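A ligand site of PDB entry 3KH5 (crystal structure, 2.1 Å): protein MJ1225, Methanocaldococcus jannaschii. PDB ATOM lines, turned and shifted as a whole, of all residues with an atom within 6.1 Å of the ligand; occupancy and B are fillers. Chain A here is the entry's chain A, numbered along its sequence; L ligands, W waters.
O1 of the ligand lies within salt-bridge range of NH2 of Arg 180 (3.8 Å).
The side-chain hydroxyl (OG1) of Thr 197 is in hydrogen-bond range of an oxygen (O2) of the ligand (3.3 Å).
The backbone NH of Ile 234 lies within hydrogen-bond range of a nitrogen (N4) of the ligand (2.8 Å).
O of Ala 256 is in hydrogen-bond range of N3 of the ligand (3.0 Å).
O6 of the ligand sits at hydrogen-bond distance from OD1 of Asp 198 (2.8 Å).
O3 of the ligand lies within salt-bridge range of NH1 of Arg 181 (2.6 Å).
O2 of the ligand is in hydrogen-bond range of OG1 of Thr 195, 3.0 Å away.
O of Ile 234 lies within hydrogen-bond range of N3 of the ligand, 3.0 Å away.
Ile 193 touches the ligand (CD1 to N2, 3.9 Å).
Lys 201 touches the ligand.
Lys 230 touches the ligand (CG to N5, 3.9 Å).
Asp 232 touches the ligand.
Val 233 touches the ligand.
Ile 254 touches the ligand.
Hydrophobic or aromatic side chains within 4 Å of the ligand: Ile 193, Val 233, Ile 234 and Ile 254.
Of the 24 residues printed, 13 come within 4 Å of the ligand.
The backbone NH (N) of Ile 193 is in hydrogen-bond range of the backbone carbonyl oxygen (O) of Lys 230, at 2.8 Å.
The side-chain carboxylate (OD2) of Asp 198 is in hydrogen-bond range of the backbone NH (N) of Thr 195.
O of Arg 180 lies within hydrogen-bond range of N of Ser 196.
N of Thr 197 lies close to OG1 of Thr 195 (3.4 Å).
Water W2 lies within hydrogen-bond range of an oxygen (O3) of the ligand, the backbone NH (N) of Gly 255 and the backbone NH (N) of Ala 256.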
ATOM      1  N   LYS A  34     -18.935  22.802  -8.614  1.00  0.00           N
ATOM      2  CA  LYS A  34     -19.517  22.028  -7.509  1.00  0.00           C
ATOM      3  C   LYS A  34     -19.917  22.905  -6.312  1.00  0.00           C
ATOM      4  O   LYS A  34     -20.394  22.400  -5.293  1.00  0.00           O
ATOM      5  CB  LYS A  34     -18.575  20.901  -7.058  1.00  0.00           C
ATOM      6  CG  LYS A  34     -19.303  19.570  -6.837  1.00  0.00           C
ATOM      7  CD  LYS A  34     -18.592  18.745  -5.754  1.00  0.00           C
ATOM      8  CE  LYS A  34     -19.234  17.367  -5.593  1.00  0.00           C
ATOM      9  NZ  LYS A  34     -20.663  17.445  -5.146  1.00  0.00           N
ATOM     10  N   ARG A  36     -22.423  25.292  -4.659  1.00  0.00           N
ATOM     11  CA  ARG A  36     -23.845  25.573  -4.727  1.00  0.00           C
ATOM     12  C   ARG A  36     -24.228  26.885  -4.002  1.00  0.00           C
ATOM     13  O   ARG A  36     -25.411  27.115  -3.724  1.00  0.00           O
ATOM     14  CB  ARG A  36     -24.638  24.363  -4.214  1.00  0.00           C
ATOM     15  CG  ARG A  36     -25.012  23.338  -5.315  1.00  0.00           C
ATOM     16  CD  ARG A  36     -23.834  22.853  -6.170  1.00  0.00           C
ATOM     17  NE  ARG A  36     -24.262  22.280  -7.451  1.00  0.00           N
ATOM     18  CZ  ARG A  36     -24.018  21.032  -7.853  1.00  0.00           C
ATOM     19  NH1 ARG A  36     -23.321  20.190  -7.082  1.00  0.00           N
ATOM     20  NH2 ARG A  36     -24.466  20.617  -9.024  1.00  0.00           N
ATOM     21  N   SER A  54     -28.582  27.214  -4.899  1.00  0.00           N
ATOM     22  CA  SER A  54     -29.456  26.268  -5.588  1.00  0.00           C
ATOM     23  C   SER A  54     -30.916  26.411  -5.166  1.00  0.00           C
ATOM     24  O   SER A  54     -31.811  26.089  -5.936  1.00  0.00           O
ATOM     25  CB  SER A  54     -28.982  24.830  -5.377  1.00  0.00           C
ATOM     26  OG  SER A  54     -28.869  24.512  -4.009  1.00  0.00           O
ATOM     27  N   ARG A 134     -19.838  23.941   7.578  1.00  0.00           N
ATOM     28  CA  ARG A 134     -18.892  22.829   7.408  1.00  0.00           C
ATOM     29  C   ARG A 134     -17.466  23.246   7.778  1.00  0.00           C
ATOM     30  O   ARG A 134     -16.761  22.499   8.446  1.00  0.00           O
ATOM     31  CB  ARG A 134     -18.944  22.279   5.968  1.00  0.00           C
ATOM     32  CG  ARG A 134     -18.254  20.912   5.773  1.00  0.00           C
ATOM     33  CD  ARG A 134     -18.807  20.118   4.574  1.00  0.00           C
ATOM     34  NE  ARG A 134     -20.271  20.129   4.515  1.00  0.00           N
ATOM     35  CZ  ARG A 134     -21.005  20.412   3.441  1.00  0.00           C
ATOM     36  NH1 ARG A 134     -20.414  20.656   2.261  1.00  0.00           N
ATOM     37  NH2 ARG A 134     -22.328  20.414   3.525  1.00  0.00           N
ATOM     38  N   ARG A 180     -33.208  22.593   2.189  1.00  0.00           N
ATOM     39  CA  ARG A 180     -32.562  22.052   0.983  1.00  0.00           C
ATOM     40  C   ARG A 180     -32.723  20.543   0.844  1.00  0.00           C
ATOM     41  O   ARG A 180     -32.680  20.021  -0.270  1.00  0.00           O
ATOM     42  CB  ARG A 180     -31.070  22.376   0.979  1.00  0.00           C
ATOM     43  CG  ARG A 180     -30.730  23.851   0.808  1.00  0.00           C
ATOM     44  CD  ARG A 180     -29.292  24.139   1.221  1.00  0.00           C
ATOM     45  NE  ARG A 180     -28.319  23.270   0.544  1.00  0.00           N
ATOM     46  CZ  ARG A 180     -26.999  23.361   0.690  1.00  0.00           C
ATOM     47  NH1 ARG A 180     -26.484  24.298   1.494  1.00  0.00           N
ATOM     48  NH2 ARG A 180     -26.199  22.537   0.038  1.00  0.00           N
ATOM     49  N   ARG A 181     -32.874  19.843   1.974  1.00  0.00           N
ATOM     50  CA  ARG A 181     -32.943  18.376   1.929  1.00  0.00           C
ATOM     51  C   ARG A 181     -34.209  17.821   2.598  1.00  0.00           C
ATOM     52  O   ARG A 181     -34.528  18.145   3.764  1.00  0.00           O
ATOM     53  CB  ARG A 181     -31.670  17.708   2.511  1.00  0.00           C
ATOM     54  CG  ARG A 181     -30.607  18.701   3.021  1.00  0.00           C
ATOM     55  CD  ARG A 181     -29.339  18.972   2.195  1.00  0.00           C
ATOM     56  NE  ARG A 181     -28.647  19.890   3.096  1.00  0.00           N
ATOM     57  CZ  ARG A 181     -27.437  20.454   2.991  1.00  0.00           C
ATOM     58  NH1 ARG A 181     -26.588  20.214   1.949  1.00  0.00           N
ATOM     59  NH2 ARG A 181     -27.071  21.299   3.986  1.00  0.00           N
ATOM     60  N   ILE A 193     -33.713  10.147  -0.316  1.00  0.00           N
ATOM     61  CA  ILE A 193     -33.514  11.543   0.027  1.00  0.00           C
ATOM     62  C   ILE A 193     -33.458  12.363  -1.271  1.00  0.00           C
ATOM     63  O   ILE A 193     -32.987  11.874  -2.305  1.00  0.00           O
ATOM     64  CB  ILE A 193     -32.229  11.757   0.882  1.00  0.00           C
ATOM     65  CG1 ILE A 193     -32.212  13.147   1.543  1.00  0.00           C
ATOM     66  CG2 ILE A 193     -30.956  11.480   0.074  1.00  0.00           C
ATOM     67  CD1 ILE A 193     -31.205  13.295   2.694  1.00  0.00           C
ATOM     68  N   ILE A 194     -33.964  13.584  -1.218  1.00  0.00           N
ATOM     69  CA  ILE A 194     -33.949  14.495  -2.357  1.00  0.00           C
ATOM     70  C   ILE A 194     -33.486  15.874  -1.860  1.00  0.00           C
ATOM     71  O   ILE A 194     -33.925  16.336  -0.799  1.00  0.00           O
ATOM     72  CB  ILE A 194     -35.345  14.546  -3.060  1.00  0.00           C
ATOM     73  CG1 ILE A 194     -35.266  15.284  -4.408  1.00  0.00           C
ATOM     74  CG2 ILE A 194     -36.420  15.170  -2.154  1.00  0.00           C
ATOM     75  CD1 ILE A 194     -34.696  14.433  -5.530  1.00  0.00           C
ATOM     76  N   THR A 195     -32.584  16.519  -2.611  1.00  0.00           N
ATOM     77  CA  THR A 195     -32.057  17.837  -2.231  1.00  0.00           C
ATOM     78  C   THR A 195     -32.169  18.827  -3.395  1.00  0.00           C
ATOM     79  O   THR A 195     -32.409  18.419  -4.527  1.00  0.00           O
ATOM     80  CB  THR A 195     -30.586  17.784  -1.712  1.00  0.00           C
ATOM     81  OG1 THR A 195     -29.676  17.640  -2.811  1.00  0.00           O
ATOM     82  CG2 THR A 195     -30.381  16.628  -0.720  1.00  0.00           C
ATOM     83  N   SER A 196     -31.993  20.120  -3.117  1.00  0.00           N
ATOM     84  CA  SER A 196     -32.044  21.155  -4.165  1.00  0.00           C
ATOM     85  C   SER A 196     -31.003  20.935  -5.270  1.00  0.00           C
ATOM     86  O   SER A 196     -31.215  21.299  -6.426  1.00  0.00           O
ATOM     87  CB  SER A 196     -31.883  22.555  -3.567  1.00  0.00           C
ATOM     88  OG  SER A 196     -30.646  22.685  -2.892  1.00  0.00           O
ATOM     89  N   THR A 197     -29.882  20.307  -4.892  1.00  0.00           N
ATOM     90  CA  THR A 197     -28.778  19.943  -5.794  1.00  0.00           C
ATOM     91  C   THR A 197     -29.235  18.969  -6.889  1.00  0.00           C
ATOM     92  O   THR A 197     -28.844  19.099  -8.061  1.00  0.00           O
ATOM     93  CB  THR A 197     -27.591  19.344  -4.978  1.00  0.00           C
ATOM     94  OG1 THR A 197     -26.906  20.398  -4.272  1.00  0.00           O
ATOM     95  CG2 THR A 197     -26.594  18.623  -5.867  1.00  0.00           C
ATOM     96  N   ASP A 198     -30.046  17.998  -6.497  1.00  0.00           N
ATOM     97  CA  ASP A 198     -30.667  17.047  -7.426  1.00  0.00           C
ATOM     98  C   ASP A 198     -31.471  17.765  -8.501  1.00  0.00           C
ATOM     99  O   ASP A 198     -31.492  17.334  -9.666  1.00  0.00           O
ATOM    100  CB  ASP A 198     -31.569  16.076  -6.667  1.00  0.00           C
ATOM    101  CG  ASP A 198     -30.796  15.162  -5.733  1.00  0.00           C
ATOM    102  OD1 ASP A 198     -29.766  14.595  -6.168  1.00  0.00           O
ATOM    103  OD2 ASP A 198     -31.213  15.000  -4.570  1.00  0.00           O
ATOM    104  N   LYS A 201     -28.957  19.309 -10.965  1.00  0.00           N
ATOM    105  CA  LYS A 201     -28.350  18.229 -11.741  1.00  0.00           C
ATOM    106  C   LYS A 201     -29.294  17.752 -12.826  1.00  0.00           C
ATOM    107  O   LYS A 201     -28.857  17.427 -13.933  1.00  0.00           O
ATOM    108  CB  LYS A 201     -27.967  17.060 -10.840  1.00  0.00           C
ATOM    109  CG  LYS A 201     -26.756  17.304  -9.949  1.00  0.00           C
ATOM    110  CD  LYS A 201     -26.554  16.122  -9.011  1.00  0.00           C
ATOM    111  CE  LYS A 201     -25.166  16.105  -8.402  1.00  0.00           C
ATOM    112  NZ  LYS A 201     -25.009  14.989  -7.427  1.00  0.00           N
ATOM    113  N   LYS A 230     -32.215   9.881  -4.416  1.00  0.00           N
ATOM    114  CA  LYS A 230     -31.163   8.987  -3.993  1.00  0.00           C
ATOM    115  C   LYS A 230     -31.813   7.977  -3.057  1.00  0.00           C
ATOM    116  O   LYS A 230     -32.289   8.348  -1.984  1.00  0.00           O
ATOM    117  CB  LYS A 230     -30.093   9.805  -3.267  1.00  0.00           C
ATOM    118  CG  LYS A 230     -28.958   9.008  -2.668  1.00  0.00           C
ATOM    119  CD  LYS A 230     -28.051   8.461  -3.751  1.00  0.00           C
ATOM    120  CE  LYS A 230     -26.822   7.823  -3.133  1.00  0.00           C
ATOM    121  NZ  LYS A 230     -26.316   6.743  -4.016  1.00  0.00           N
ATOM    122  N   ASP A 232     -30.415   5.244  -1.614  1.00  0.00           N
ATOM    123  CA  ASP A 232     -29.570   4.783  -0.530  1.00  0.00           C
ATOM    124  C   ASP A 232     -29.006   5.944   0.263  1.00  0.00           C
ATOM    125  O   ASP A 232     -28.121   6.684  -0.196  1.00  0.00           O
ATOM    126  CB  ASP A 232     -28.524   3.816  -1.052  1.00  0.00           C
ATOM    127  CG  ASP A 232     -29.153   2.538  -1.583  1.00  0.00           C
ATOM    128  OD1 ASP A 232     -29.528   1.662  -0.776  1.00  0.00           O
ATOM    129  OD2 ASP A 232     -29.285   2.425  -2.814  1.00  0.00           O
ATOM    130  N   VAL A 233     -29.546   6.101   1.467  1.00  0.00           N
ATOM    131  CA  VAL A 233     -29.315   7.288   2.272  1.00  0.00           C
ATOM    132  C   VAL A 233     -28.376   6.970   3.415  1.00  0.00           C
ATOM    133  O   VAL A 233     -28.461   5.904   4.030  1.00  0.00           O
ATOM    134  CB  VAL A 233     -30.657   7.830   2.833  1.00  0.00           C
ATOM    135  CG1 VAL A 233     -30.478   9.244   3.364  1.00  0.00           C
ATOM    136  CG2 VAL A 233     -31.737   7.800   1.770  1.00  0.00           C
ATOM    137  N   ILE A 234     -27.458   7.896   3.702  1.00  0.00           N
ATOM    138  CA  ILE A 234     -26.644   7.847   4.904  1.00  0.00           C
ATOM    139  C   ILE A 234     -27.501   8.418   6.036  1.00  0.00           C
ATOM    140  O   ILE A 234     -27.923   9.579   5.981  1.00  0.00           O
ATOM    141  CB  ILE A 234     -25.331   8.640   4.744  1.00  0.00           C
ATOM    142  CG1 ILE A 234     -24.481   8.013   3.624  1.00  0.00           C
ATOM    143  CG2 ILE A 234     -24.553   8.675   6.059  1.00  0.00           C
ATOM    144  CD1 ILE A 234     -23.425   8.934   3.056  1.00  0.00           C
ATOM    145  N   THR A 235     -27.748   7.585   7.053  1.00  0.00           N
ATOM    146  CA  THR A 235     -28.670   7.908   8.137  1.00  0.00           C
ATOM    147  C   THR A 235     -27.948   7.949   9.489  1.00  0.00           C
ATOM    148  O   THR A 235     -26.826   7.441   9.613  1.00  0.00           O
ATOM    149  CB  THR A 235     -29.807   6.860   8.230  1.00  0.00           C
ATOM    150  OG1 THR A 235     -29.251   5.570   8.533  1.00  0.00           O
ATOM    151  CG2 THR A 235     -30.566   6.777   6.918  1.00  0.00           C
ATOM    152  N   ASP A 253     -18.953  16.088   2.597  1.00  0.00           N
ATOM    153  CA  ASP A 253     -19.699  17.251   2.123  1.00  0.00           C
ATOM    154  C   ASP A 253     -21.199  16.960   2.078  1.00  0.00           C
ATOM    155  O   ASP A 253     -21.856  17.186   1.061  1.00  0.00           O
ATOM    156  CB  ASP A 253     -19.243  17.661   0.718  1.00  0.00           C
ATOM    157  CG  ASP A 253     -17.868  18.311   0.694  1.00  0.00           C
ATOM    158  OD1 ASP A 253     -17.538  19.092   1.621  1.00  0.00           O
ATOM    159  OD2 ASP A 253     -17.112  18.060  -0.276  1.00  0.00           O
ATOM    160  N   ILE A 254     -21.732  16.410   3.173  1.00  0.00           N
ATOM    161  CA  ILE A 254     -23.168  16.152   3.297  1.00  0.00           C
ATOM    162  C   ILE A 254     -23.602  17.029   4.459  1.00  0.00           C
ATOM    163  O   ILE A 254     -22.836  17.224   5.405  1.00  0.00           O
ATOM    164  CB  ILE A 254     -23.423  14.638   3.579  1.00  0.00           C
ATOM    165  CG1 ILE A 254     -23.233  13.818   2.295  1.00  0.00           C
ATOM    166  CG2 ILE A 254     -24.831  14.391   4.156  1.00  0.00           C
ATOM    167  CD1 ILE A 254     -22.987  12.331   2.548  1.00  0.00           C
ATOM    168  N   GLY A 255     -24.802  17.603   4.380  1.00  0.00           N
ATOM    169  CA  GLY A 255     -25.246  18.526   5.417  1.00  0.00           C
ATOM    170  C   GLY A 255     -26.341  17.995   6.318  1.00  0.00           C
ATOM    171  O   GLY A 255     -26.626  18.586   7.358  1.00  0.00           O
ATOM    172  N   ALA A 256     -26.950  16.866   5.933  1.00  0.00           N
ATOM    173  CA  ALA A 256     -28.110  16.341   6.642  1.00  0.00           C
ATOM    174  C   ALA A 256     -28.200  14.820   6.606  1.00  0.00           C
ATOM    175  O   ALA A 256     -28.061  14.207   5.535  1.00  0.00           O
ATOM    176  CB  ALA A 256     -29.400  16.957   6.082  1.00  0.00           C
ATOM    177  N   LEU A 257     -28.434  14.207   7.765  1.00  0.00           N
ATOM    178  CA  LEU A 257     -28.747  12.779   7.860  1.00  0.00           C
ATOM    179  C   LEU A 257     -30.133  12.585   8.473  1.00  0.00           C
ATOM    180  O   LEU A 257     -30.419  13.125   9.553  1.00  0.00           O
ATOM    181  CB  LEU A 257     -27.693  12.029   8.688  1.00  0.00           C
ATOM    182  CG  LEU A 257     -26.254  11.834   8.185  1.00  0.00           C
ATOM    183  CD1 LEU A 257     -25.500  13.145   8.058  1.00  0.00           C
ATOM    184  CD2 LEU A 257     -25.490  10.901   9.132  1.00  0.00           C
ATOM    185  N   PRO A 258     -31.023  11.840   7.774  1.00  0.00           N
ATOM    186  CA  PRO A 258     -32.280  11.406   8.373  1.00  0.00           C
ATOM    187  C   PRO A 258     -31.968  10.478   9.547  1.00  0.00           C
ATOM    188  O   PRO A 258     -31.039   9.677   9.457  1.00  0.00           O
ATOM    189  CB  PRO A 258     -32.949  10.624   7.233  1.00  0.00           C
ATOM    190  CG  PRO A 258     -32.361  11.192   5.986  1.00  0.00           C
ATOM    191  CD  PRO A 258     -30.930  11.475   6.349  1.00  0.00           C
HETATM  192  P1  LIG L   1     -26.313  18.426  -1.033  1.00  0.00           P
HETATM  193  O1  LIG L   1     -25.144  19.241  -1.456  1.00  0.00           O
HETATM  194  O2  LIG L   1     -27.696  19.228  -1.245  1.00  0.00           O
HETATM  195  O3  LIG L   1     -26.272  18.062   0.549  1.00  0.00           O
HETATM  196  O4  LIG L   1     -26.471  17.045  -1.836  1.00  0.00           O
HETATM  197  C1  LIG L   1     -25.504  16.566  -2.806  1.00  0.00           C
HETATM  198  C2  LIG L   1     -25.808  15.115  -3.163  1.00  0.00           C
HETATM  199  O5  LIG L   1     -25.698  14.372  -1.909  1.00  0.00           O
HETATM  200  C3  LIG L   1     -27.289  15.047  -3.612  1.00  0.00           C
HETATM  201  O6  LIG L   1     -27.436  14.131  -4.712  1.00  0.00           O
HETATM  202  C4  LIG L   1     -28.004  14.508  -2.373  1.00  0.00           C
HETATM  203  O7  LIG L   1     -29.127  13.719  -2.763  1.00  0.00           O
HETATM  204  C5  LIG L   1     -26.925  13.643  -1.717  1.00  0.00           C
HETATM  205  N1  LIG L   1     -27.139  13.477  -0.251  1.00  0.00           N
HETATM  206  C6  LIG L   1     -27.346  14.443   0.646  1.00  0.00           C
HETATM  207  N2  LIG L   1     -27.496  13.918   1.855  1.00  0.00           N
HETATM  208  C7  LIG L   1     -27.373  12.597   1.731  1.00  0.00           C
HETATM  209  C8  LIG L   1     -27.421  11.540   2.632  1.00  0.00           C
HETATM  210  N3  LIG L   1     -27.647  11.770   3.916  1.00  0.00           N
HETATM  211  N4  LIG L   1     -27.242  10.282   2.168  1.00  0.00           N
HETATM  212  C9  LIG L   1     -27.023  10.046   0.880  1.00  0.00           C
HETATM  213  N5  LIG L   1     -26.963  11.036  -0.004  1.00  0.00           N
HETATM  214  C10 LIG L   1     -27.138  12.312   0.388  1.00  0.00           C
HETATM  215  O   HOH W   1     -24.838  10.391  -2.196  1.00  0.00           O
HETATM  216  O   HOH W   2     -26.884  16.753   2.773  1.00  0.00           O
